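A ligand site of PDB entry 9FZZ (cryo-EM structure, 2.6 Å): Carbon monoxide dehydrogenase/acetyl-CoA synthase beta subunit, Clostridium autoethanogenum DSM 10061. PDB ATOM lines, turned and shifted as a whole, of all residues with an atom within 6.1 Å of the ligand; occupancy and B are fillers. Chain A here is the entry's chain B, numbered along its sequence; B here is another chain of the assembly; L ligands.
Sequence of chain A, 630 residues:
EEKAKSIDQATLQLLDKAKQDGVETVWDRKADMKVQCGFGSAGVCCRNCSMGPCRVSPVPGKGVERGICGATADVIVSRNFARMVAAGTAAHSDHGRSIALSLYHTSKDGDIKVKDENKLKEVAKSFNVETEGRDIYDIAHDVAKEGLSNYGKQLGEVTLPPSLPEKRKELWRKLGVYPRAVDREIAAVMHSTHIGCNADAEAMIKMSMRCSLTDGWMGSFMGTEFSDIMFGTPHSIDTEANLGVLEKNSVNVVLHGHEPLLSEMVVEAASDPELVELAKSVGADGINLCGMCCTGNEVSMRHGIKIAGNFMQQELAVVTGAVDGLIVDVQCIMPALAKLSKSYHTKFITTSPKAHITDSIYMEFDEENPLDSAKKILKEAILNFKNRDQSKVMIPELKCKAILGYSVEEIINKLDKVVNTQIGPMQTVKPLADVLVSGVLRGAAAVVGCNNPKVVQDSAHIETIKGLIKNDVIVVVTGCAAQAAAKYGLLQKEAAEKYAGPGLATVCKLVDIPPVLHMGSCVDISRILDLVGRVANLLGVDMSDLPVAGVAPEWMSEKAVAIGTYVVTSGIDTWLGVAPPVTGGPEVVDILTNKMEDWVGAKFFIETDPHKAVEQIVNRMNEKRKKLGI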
ATOM      1  N   HIS A  92      22.643 -13.708  -8.876  1.00  0.00           N
ATOM      2  CA  HIS A  92      22.601 -14.546  -7.676  1.00  0.00           C
ATOM      3  C   HIS A  92      22.128 -13.772  -6.440  1.00  0.00           C
ATOM      4  O   HIS A  92      21.336 -14.274  -5.644  1.00  0.00           O
ATOM      5  CB  HIS A  92      23.967 -15.190  -7.429  1.00  0.00           C
ATOM      6  CG  HIS A  92      24.225 -16.395  -8.273  1.00  0.00           C
ATOM      7  ND1 HIS A  92      25.453 -16.694  -8.787  1.00  0.00           N
ATOM      8  CD2 HIS A  92      23.390 -17.370  -8.705  1.00  0.00           C
ATOM      9  CE1 HIS A  92      25.370 -17.806  -9.506  1.00  0.00           C
ATOM     10  NE2 HIS A  92      24.117 -18.229  -9.464  1.00  0.00           N
ATOM     11  N   GLY A 257      13.265 -21.983 -14.639  1.00  0.00           N
ATOM     12  CA  GLY A 257      13.736 -20.788 -13.959  1.00  0.00           C
ATOM     13  C   GLY A 257      14.585 -21.078 -12.729  1.00  0.00           C
ATOM     14  O   GLY A 257      15.254 -22.111 -12.667  1.00  0.00           O
ATOM     15  N   HIS A 258      14.619 -20.137 -11.771  1.00  0.00           N
ATOM     16  CA  HIS A 258      15.536 -20.256 -10.648  1.00  0.00           C
ATOM     17  C   HIS A 258      14.924 -20.033  -9.267  1.00  0.00           C
ATOM     18  O   HIS A 258      15.376 -20.637  -8.284  1.00  0.00           O
ATOM     19  CB  HIS A 258      16.716 -19.302 -10.850  1.00  0.00           C
ATOM     20  CG  HIS A 258      17.661 -19.742 -11.936  1.00  0.00           C
ATOM     21  ND1 HIS A 258      17.345 -19.715 -13.258  1.00  0.00           N
ATOM     22  CD2 HIS A 258      18.908 -20.273 -11.861  1.00  0.00           C
ATOM     23  CE1 HIS A 258      18.342 -20.194 -13.980  1.00  0.00           C
ATOM     24  NE2 HIS A 258      19.309 -20.541 -13.138  1.00  0.00           N
ATOM     25  N   CYS A 293      16.175 -26.961 -15.340  1.00  0.00           N
ATOM     26  CA  CYS A 293      17.242 -26.051 -14.868  1.00  0.00           C
ATOM     27  C   CYS A 293      17.175 -25.997 -13.337  1.00  0.00           C
ATOM     28  O   CYS A 293      16.909 -27.011 -12.688  1.00  0.00           O
ATOM     29  CB  CYS A 293      17.100 -24.699 -15.566  1.00  0.00           C
ATOM     30  SG  CYS A 293      17.477 -24.703 -17.342  1.00  0.00           S
ATOM     31  N   CYS A 294      17.433 -24.833 -12.743  1.00  0.00           N
ATOM     32  CA  CYS A 294      17.676 -24.746 -11.297  1.00  0.00           C
ATOM     33  C   CYS A 294      16.400 -24.871 -10.473  1.00  0.00           C
ATOM     34  O   CYS A 294      16.436 -25.428  -9.381  1.00  0.00           O
ATOM     35  CB  CYS A 294      18.405 -23.454 -10.955  1.00  0.00           C
ATOM     36  SG  CYS A 294      20.160 -23.568 -11.316  1.00  0.00           S
ATOM     37  N   ASN A 310      17.873 -29.909 -18.903  1.00  0.00           N
ATOM     38  CA  ASN A 310      18.701 -28.748 -18.581  1.00  0.00           C
ATOM     39  C   ASN A 310      18.543 -27.658 -19.648  1.00  0.00           C
ATOM     40  O   ASN A 310      17.653 -27.713 -20.502  1.00  0.00           O
ATOM     41  CB  ASN A 310      20.163 -29.155 -18.337  1.00  0.00           C
ATOM     42  CG  ASN A 310      20.753 -30.046 -19.432  1.00  0.00           C
ATOM     43  OD1 ASN A 310      20.152 -30.207 -20.486  1.00  0.00           O
ATOM     44  ND2 ASN A 310      21.936 -30.617 -19.183  1.00  0.00           N
ATOM     45  N   PHE A 311      19.434 -26.667 -19.631  1.00  0.00           N
ATOM     46  CA  PHE A 311      19.280 -25.411 -20.373  1.00  0.00           C
ATOM     47  C   PHE A 311      18.943 -25.658 -21.845  1.00  0.00           C
ATOM     48  O   PHE A 311      17.850 -25.303 -22.294  1.00  0.00           O
ATOM     49  CB  PHE A 311      20.553 -24.566 -20.223  1.00  0.00           C
ATOM     50  CG  PHE A 311      20.528 -23.259 -20.998  1.00  0.00           C
ATOM     51  CD1 PHE A 311      19.651 -22.227 -20.626  1.00  0.00           C
ATOM     52  CD2 PHE A 311      21.381 -23.067 -22.083  1.00  0.00           C
ATOM     53  CE1 PHE A 311      19.618 -21.003 -21.341  1.00  0.00           C
ATOM     54  CE2 PHE A 311      21.372 -21.844 -22.813  1.00  0.00           C
ATOM     55  CZ  PHE A 311      20.483 -20.811 -22.433  1.00  0.00           C
ATOM     56  N   GLN A 331      15.785 -15.824 -15.331  1.00  0.00           N
ATOM     57  CA  GLN A 331      17.138 -16.315 -15.588  1.00  0.00           C
ATOM     58  C   GLN A 331      17.139 -17.576 -16.464  1.00  0.00           C
ATOM     59  O   GLN A 331      16.400 -18.533 -16.203  1.00  0.00           O
ATOM     60  CB  GLN A 331      17.902 -16.577 -14.280  1.00  0.00           C
ATOM     61  CG  GLN A 331      18.110 -15.317 -13.408  1.00  0.00           C
ATOM     62  CD  GLN A 331      18.823 -15.640 -12.086  1.00  0.00           C
ATOM     63  OE1 GLN A 331      19.531 -16.636 -11.987  1.00  0.00           O
ATOM     64  NE2 GLN A 331      18.612 -14.813 -11.067  1.00  0.00           N
ATOM     65  N   CYS A 332      17.976 -17.581 -17.508  1.00  0.00           N
ATOM     66  CA  CYS A 332      18.184 -18.760 -18.369  1.00  0.00           C
ATOM     67  C   CYS A 332      16.893 -19.241 -19.029  1.00  0.00           C
ATOM     68  O   CYS A 332      16.739 -20.422 -19.342  1.00  0.00           O
ATOM     69  CB  CYS A 332      18.849 -19.898 -17.596  1.00  0.00           C
ATOM     70  SG  CYS A 332      20.356 -19.362 -16.748  1.00  0.00           S
ATOM     71  N   VAL A 448      30.063 -28.063 -12.517  1.00  0.00           N
ATOM     72  CA  VAL A 448      28.994 -27.078 -12.505  1.00  0.00           C
ATOM     73  C   VAL A 448      28.906 -26.453 -13.892  1.00  0.00           C
ATOM     74  O   VAL A 448      29.788 -26.640 -14.734  1.00  0.00           O
ATOM     75  CB  VAL A 448      29.236 -25.981 -11.437  1.00  0.00           C
ATOM     76  CG1 VAL A 448      29.597 -26.621 -10.099  1.00  0.00           C
ATOM     77  CG2 VAL A 448      30.347 -25.024 -11.888  1.00  0.00           C
ATOM     78  N   GLY A 449      27.844 -25.706 -14.141  1.00  0.00           N
ATOM     79  CA  GLY A 449      27.783 -24.892 -15.335  1.00  0.00           C
ATOM     80  C   GLY A 449      26.645 -25.299 -16.244  1.00  0.00           C
ATOM     81  O   GLY A 449      25.924 -26.268 -16.008  1.00  0.00           O
ATOM     82  N   CYS A 450      26.536 -24.565 -17.347  1.00  0.00           N
ATOM     83  CA  CYS A 450      25.444 -24.652 -18.294  1.00  0.00           C
ATOM     84  C   CYS A 450      25.795 -25.554 -19.464  1.00  0.00           C
ATOM     85  O   CYS A 450      26.758 -26.334 -19.416  1.00  0.00           O
ATOM     86  CB  CYS A 450      25.181 -23.241 -18.825  1.00  0.00           C
ATOM     87  SG  CYS A 450      25.760 -21.905 -17.735  1.00  0.00           S
ATOM     88  N   ASN A 451      24.990 -25.492 -20.518  1.00  0.00           N
ATOM     89  CA  ASN A 451      25.327 -25.990 -21.836  1.00  0.00           C
ATOM     90  C   ASN A 451      25.753 -24.783 -22.674  1.00  0.00           C
ATOM     91  O   ASN A 451      25.545 -23.627 -22.280  1.00  0.00           O
ATOM     92  CB  ASN A 451      24.172 -26.728 -22.500  1.00  0.00           C
ATOM     93  CG  ASN A 451      23.665 -27.901 -21.679  1.00  0.00           C
ATOM     94  OD1 ASN A 451      22.481 -28.007 -21.406  1.00  0.00           O
ATOM     95  ND2 ASN A 451      24.577 -28.807 -21.284  1.00  0.00           N
ATOM     96  N   THR A 478      26.351 -29.683  -9.721  1.00  0.00           N
ATOM     97  CA  THR A 478      25.234 -28.749  -9.548  1.00  0.00           C
ATOM     98  C   THR A 478      24.701 -28.323 -10.918  1.00  0.00           C
ATOM     99  O   THR A 478      25.375 -28.443 -11.939  1.00  0.00           O
ATOM    100  CB  THR A 478      25.593 -27.491  -8.740  1.00  0.00           C
ATOM    101  OG1 THR A 478      26.528 -26.679  -9.461  1.00  0.00           O
ATOM    102  CG2 THR A 478      26.178 -27.866  -7.383  1.00  0.00           C
ATOM    103  N   GLY A 479      23.449 -27.873 -10.910  1.00  0.00           N
ATOM    104  CA  GLY A 479      22.894 -27.198 -12.076  1.00  0.00           C
ATOM    105  C   GLY A 479      22.718 -28.090 -13.298  1.00  0.00           C
ATOM    106  O   GLY A 479      22.364 -29.275 -13.206  1.00  0.00           O
ATOM    107  N   CYS A 480      22.968 -27.491 -14.464  1.00  0.00           N
ATOM    108  CA  CYS A 480      22.755 -28.207 -15.717  1.00  0.00           C
ATOM    109  C   CYS A 480      23.744 -29.359 -15.887  1.00  0.00           C
ATOM    110  O   CYS A 480      23.419 -30.367 -16.509  1.00  0.00           O
ATOM    111  CB  CYS A 480      22.829 -27.212 -16.886  1.00  0.00           C
ATOM    112  SG  CYS A 480      21.350 -26.135 -16.957  1.00  0.00           S
ATOM    113  N   ALA A 481      24.956 -29.239 -15.329  1.00  0.00           N
ATOM    114  CA  ALA A 481      25.877 -30.375 -15.290  1.00  0.00           C
ATOM    115  C   ALA A 481      25.309 -31.521 -14.478  1.00  0.00           C
ATOM    116  O   ALA A 481      25.350 -32.689 -14.906  1.00  0.00           O
ATOM    117  CB  ALA A 481      27.228 -29.934 -14.723  1.00  0.00           C
ATOM    118  N   GLN A 483      22.180 -32.105 -14.042  1.00  0.00           N
ATOM    119  CA  GLN A 483      21.087 -32.676 -14.835  1.00  0.00           C
ATOM    120  C   GLN A 483      21.607 -33.509 -15.999  1.00  0.00           C
ATOM    121  O   GLN A 483      21.021 -34.541 -16.334  1.00  0.00           O
ATOM    122  CB  GLN A 483      20.128 -31.557 -15.280  1.00  0.00           C
ATOM    123  CG  GLN A 483      19.401 -30.926 -14.054  1.00  0.00           C
ATOM    124  CD  GLN A 483      18.519 -29.708 -14.385  1.00  0.00           C
ATOM    125  OE1 GLN A 483      18.697 -29.072 -15.408  1.00  0.00           O
ATOM    126  NE2 GLN A 483      17.573 -29.395 -13.493  1.00  0.00           N
ATOM    127  N   SER A 521      21.113 -26.760  -6.969  1.00  0.00           N
ATOM    128  CA  SER A 521      21.095 -25.754  -8.029  1.00  0.00           C
ATOM    129  C   SER A 521      22.404 -24.970  -8.039  1.00  0.00           C
ATOM    130  O   SER A 521      23.355 -25.287  -7.341  1.00  0.00           O
ATOM    131  CB  SER A 521      19.875 -24.844  -7.851  1.00  0.00           C
ATOM    132  OG  SER A 521      19.974 -24.080  -6.655  1.00  0.00           O
ATOM    133  N   CYS A 522      22.443 -23.909  -8.860  1.00  0.00           N
ATOM    134  CA  CYS A 522      23.652 -23.093  -8.975  1.00  0.00           C
ATOM    135  C   CYS A 522      23.953 -22.355  -7.668  1.00  0.00           C
ATOM    136  O   CYS A 522      25.109 -22.305  -7.231  1.00  0.00           O
ATOM    137  CB  CYS A 522      23.514 -22.139 -10.155  1.00  0.00           C
ATOM    138  SG  CYS A 522      23.602 -23.054 -11.699  1.00  0.00           S
ATOM    139  N   MET A 556      27.944 -20.942 -20.045  1.00  0.00           N
ATOM    140  CA  MET A 556      27.524 -19.871 -20.941  1.00  0.00           C
ATOM    141  C   MET A 556      27.212 -18.546 -20.241  1.00  0.00           C
ATOM    142  O   MET A 556      27.397 -17.488 -20.834  1.00  0.00           O
ATOM    143  CB  MET A 556      26.322 -20.333 -21.788  1.00  0.00           C
ATOM    144  CG  MET A 556      24.996 -20.476 -21.006  1.00  0.00           C
ATOM    145  SD  MET A 556      23.969 -18.997 -20.867  1.00  0.00           S
ATOM    146  CE  MET A 556      22.650 -19.565 -19.790  1.00  0.00           C
ATOM    147  N   SER A 557      26.748 -18.587 -18.985  1.00  0.00           N
ATOM    148  CA  SER A 557      26.124 -17.436 -18.349  1.00  0.00           C
ATOM    149  C   SER A 557      27.136 -16.564 -17.616  1.00  0.00           C
ATOM    150  O   SER A 557      28.231 -16.998 -17.230  1.00  0.00           O
ATOM    151  CB  SER A 557      25.017 -17.876 -17.366  1.00  0.00           C
ATOM    152  OG  SER A 557      25.542 -18.611 -16.263  1.00  0.00           O
ATOM    153  N   LYS A 559      26.521 -15.643 -14.672  1.00  0.00           N
ATOM    154  CA  LYS A 559      26.552 -16.302 -13.370  1.00  0.00           C
ATOM    155  C   LYS A 559      27.699 -17.310 -13.284  1.00  0.00           C
ATOM    156  O   LYS A 559      28.409 -17.352 -12.269  1.00  0.00           O
ATOM    157  CB  LYS A 559      25.230 -17.011 -13.101  1.00  0.00           C
ATOM    158  CG  LYS A 559      24.111 -16.083 -12.605  1.00  0.00           C
ATOM    159  CD  LYS A 559      22.815 -16.871 -12.330  1.00  0.00           C
ATOM    160  CE  LYS A 559      22.192 -17.403 -13.657  1.00  0.00           C
ATOM    161  NZ  LYS A 559      21.005 -18.315 -13.441  1.00  0.00           N
ATOM    162  N   ALA A 560      27.959 -18.051 -14.353  1.00  0.00           N
ATOM    163  CA  ALA A 560      29.073 -18.993 -14.358  1.00  0.00           C
ATOM    164  C   ALA A 560      30.405 -18.275 -14.197  1.00  0.00           C
ATOM    165  O   ALA A 560      31.305 -18.756 -13.493  1.00  0.00           O
ATOM    166  CB  ALA A 560      29.054 -19.825 -15.638  1.00  0.00           C
ATOM    167  N   ILE A 563      30.736 -17.334 -10.599  1.00  0.00           N
ATOM    168  CA  ILE A 563      30.967 -18.550  -9.809  1.00  0.00           C
ATOM    169  C   ILE A 563      32.423 -18.971  -9.890  1.00  0.00           C
ATOM    170  O   ILE A 563      33.084 -19.206  -8.864  1.00  0.00           O
ATOM    171  CB  ILE A 563      30.039 -19.684 -10.267  1.00  0.00           C
ATOM    172  CG1 ILE A 563      28.602 -19.433  -9.816  1.00  0.00           C
ATOM    173  CG2 ILE A 563      30.532 -21.066  -9.751  1.00  0.00           C
ATOM    174  CD1 ILE A 563      27.606 -20.279 -10.579  1.00  0.00           C
ATOM    175  N   HIS B 194      20.612  -9.993 -17.542  1.00  0.00           N
ATOM    176  CA  HIS B 194      21.276 -11.292 -17.657  1.00  0.00           C
ATOM    177  C   HIS B 194      20.558 -12.180 -18.673  1.00  0.00           C
ATOM    178  O   HIS B 194      19.347 -12.079 -18.872  1.00  0.00           O
ATOM    179  CB  HIS B 194      21.286 -11.962 -16.276  1.00  0.00           C
ATOM    180  CG  HIS B 194      22.033 -13.266 -16.232  1.00  0.00           C
ATOM    181  ND1 HIS B 194      21.514 -14.434 -16.699  1.00  0.00           N
ATOM    182  CD2 HIS B 194      23.265 -13.559 -15.742  1.00  0.00           C
ATOM    183  CE1 HIS B 194      22.396 -15.412 -16.523  1.00  0.00           C
ATOM    184  NE2 HIS B 194      23.466 -14.900 -15.938  1.00  0.00           N
HETATM  185 FE1  LIG L   1      21.434 -21.353 -16.141  1.00  0.00          FE
HETATM  186 FE2  LIG L   1      20.718 -22.043 -12.909  1.00  0.00          FE
HETATM  187 FE3  LIG L   1      23.907 -22.296 -16.378  1.00  0.00          FE
HETATM  188 FE4  LIG L   1      21.909 -24.160 -16.141  1.00  0.00          FE
HETATM  189  S1  LIG L   1      23.790 -23.955 -14.804  1.00  0.00           S
HETATM  190  S2  LIG L   1      22.253 -22.667 -17.893  1.00  0.00           S
HETATM  191  S3  LIG L   1      23.313 -20.395 -15.138  1.00  0.00           S
HETATM  192  S4  LIG L   1      20.261 -22.900 -15.037  1.00  0.00           S
HETATM  193 NI1  LIG L   1      23.141 -22.152 -13.525  1.00  0.00          NI
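An iron atom (FE2) of the ligand is bound by a ring nitrogen (NE2) of His 258 (2.1 Å).
NI1 of the ligand is bound by SG of Cys 522, 2.1 Å away.
A sulfur (S1) of the ligand lies close to the backbone NH (N) of Cys 480, 3.6 Å away.
The side-chain sulfur (SG) of Cys 480 binds an iron atom (FE4) of the ligand (2.2 Å).
An iron atom (FE2) of the ligand is bound by the side-chain sulfur of Cys 294.
N of Cys 450 sits close to S1 of the ligand, 3.8 Å away.
The side-chain sulfur of Cys 450 is bound to an iron atom (FE3) of the ligand, at 2.3 Å.
The side-chain sulfur (SG) of Cys 332 binds an iron atom (FE1) of the ligand (2.3 Å).
A sulfur (S3) of the ligand lies close to the side-chain hydroxyl (OG) of Ser 557 (3.1 Å).
NZ of Lys 559 lies close to S3 of the ligand (3.5 Å).
NE2 of His 258 lies close to NZ of Lys 559, at 2.8 Å.
The backbone NH of Cys 522 sits close to the side-chain sulfur of Cys 294 (3.4 Å).
The backbone carbonyl oxygen of Cys 480 sits at hydrogen-bond distance from the side-chain amide nitrogen of Asn 310 (3.1 Å).
SG of Cys 450 sits close to N of Met 556 (3.3 Å).
SG of Cys 332 sits close to NZ of Lys 559 (3.5 Å).
O of Gly 449 sits at hydrogen-bond distance from N of Ala 481, 3.2 Å away.
The side-chain sulfur (SG) of Cys 293 is in hydrogen-bond range of the backbone NH (N) of Phe 311, at 3.6 Å.
N of Lys 559 lies within hydrogen-bond range of NE2 of His 194 of chain B, 3.4 Å away.
A sulfur (S1) of the ligand lies close to the backbone carbonyl oxygen of Gly 449.
Residues that only touch the ligand: Cys 293 (3.7 Å), Phe 311 (3.5 Å) and Met 556 (3.7 Å).
Hydrophobic or aromatic side chains within 4 Å of the ligand: His 258, Phe 311 and Met 556.
Of the 26 residues printed, 12 come within 4 Å of the ligand.
The nearest printed residue that does not touch the ligand is Gly 479 (4.3 Å).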
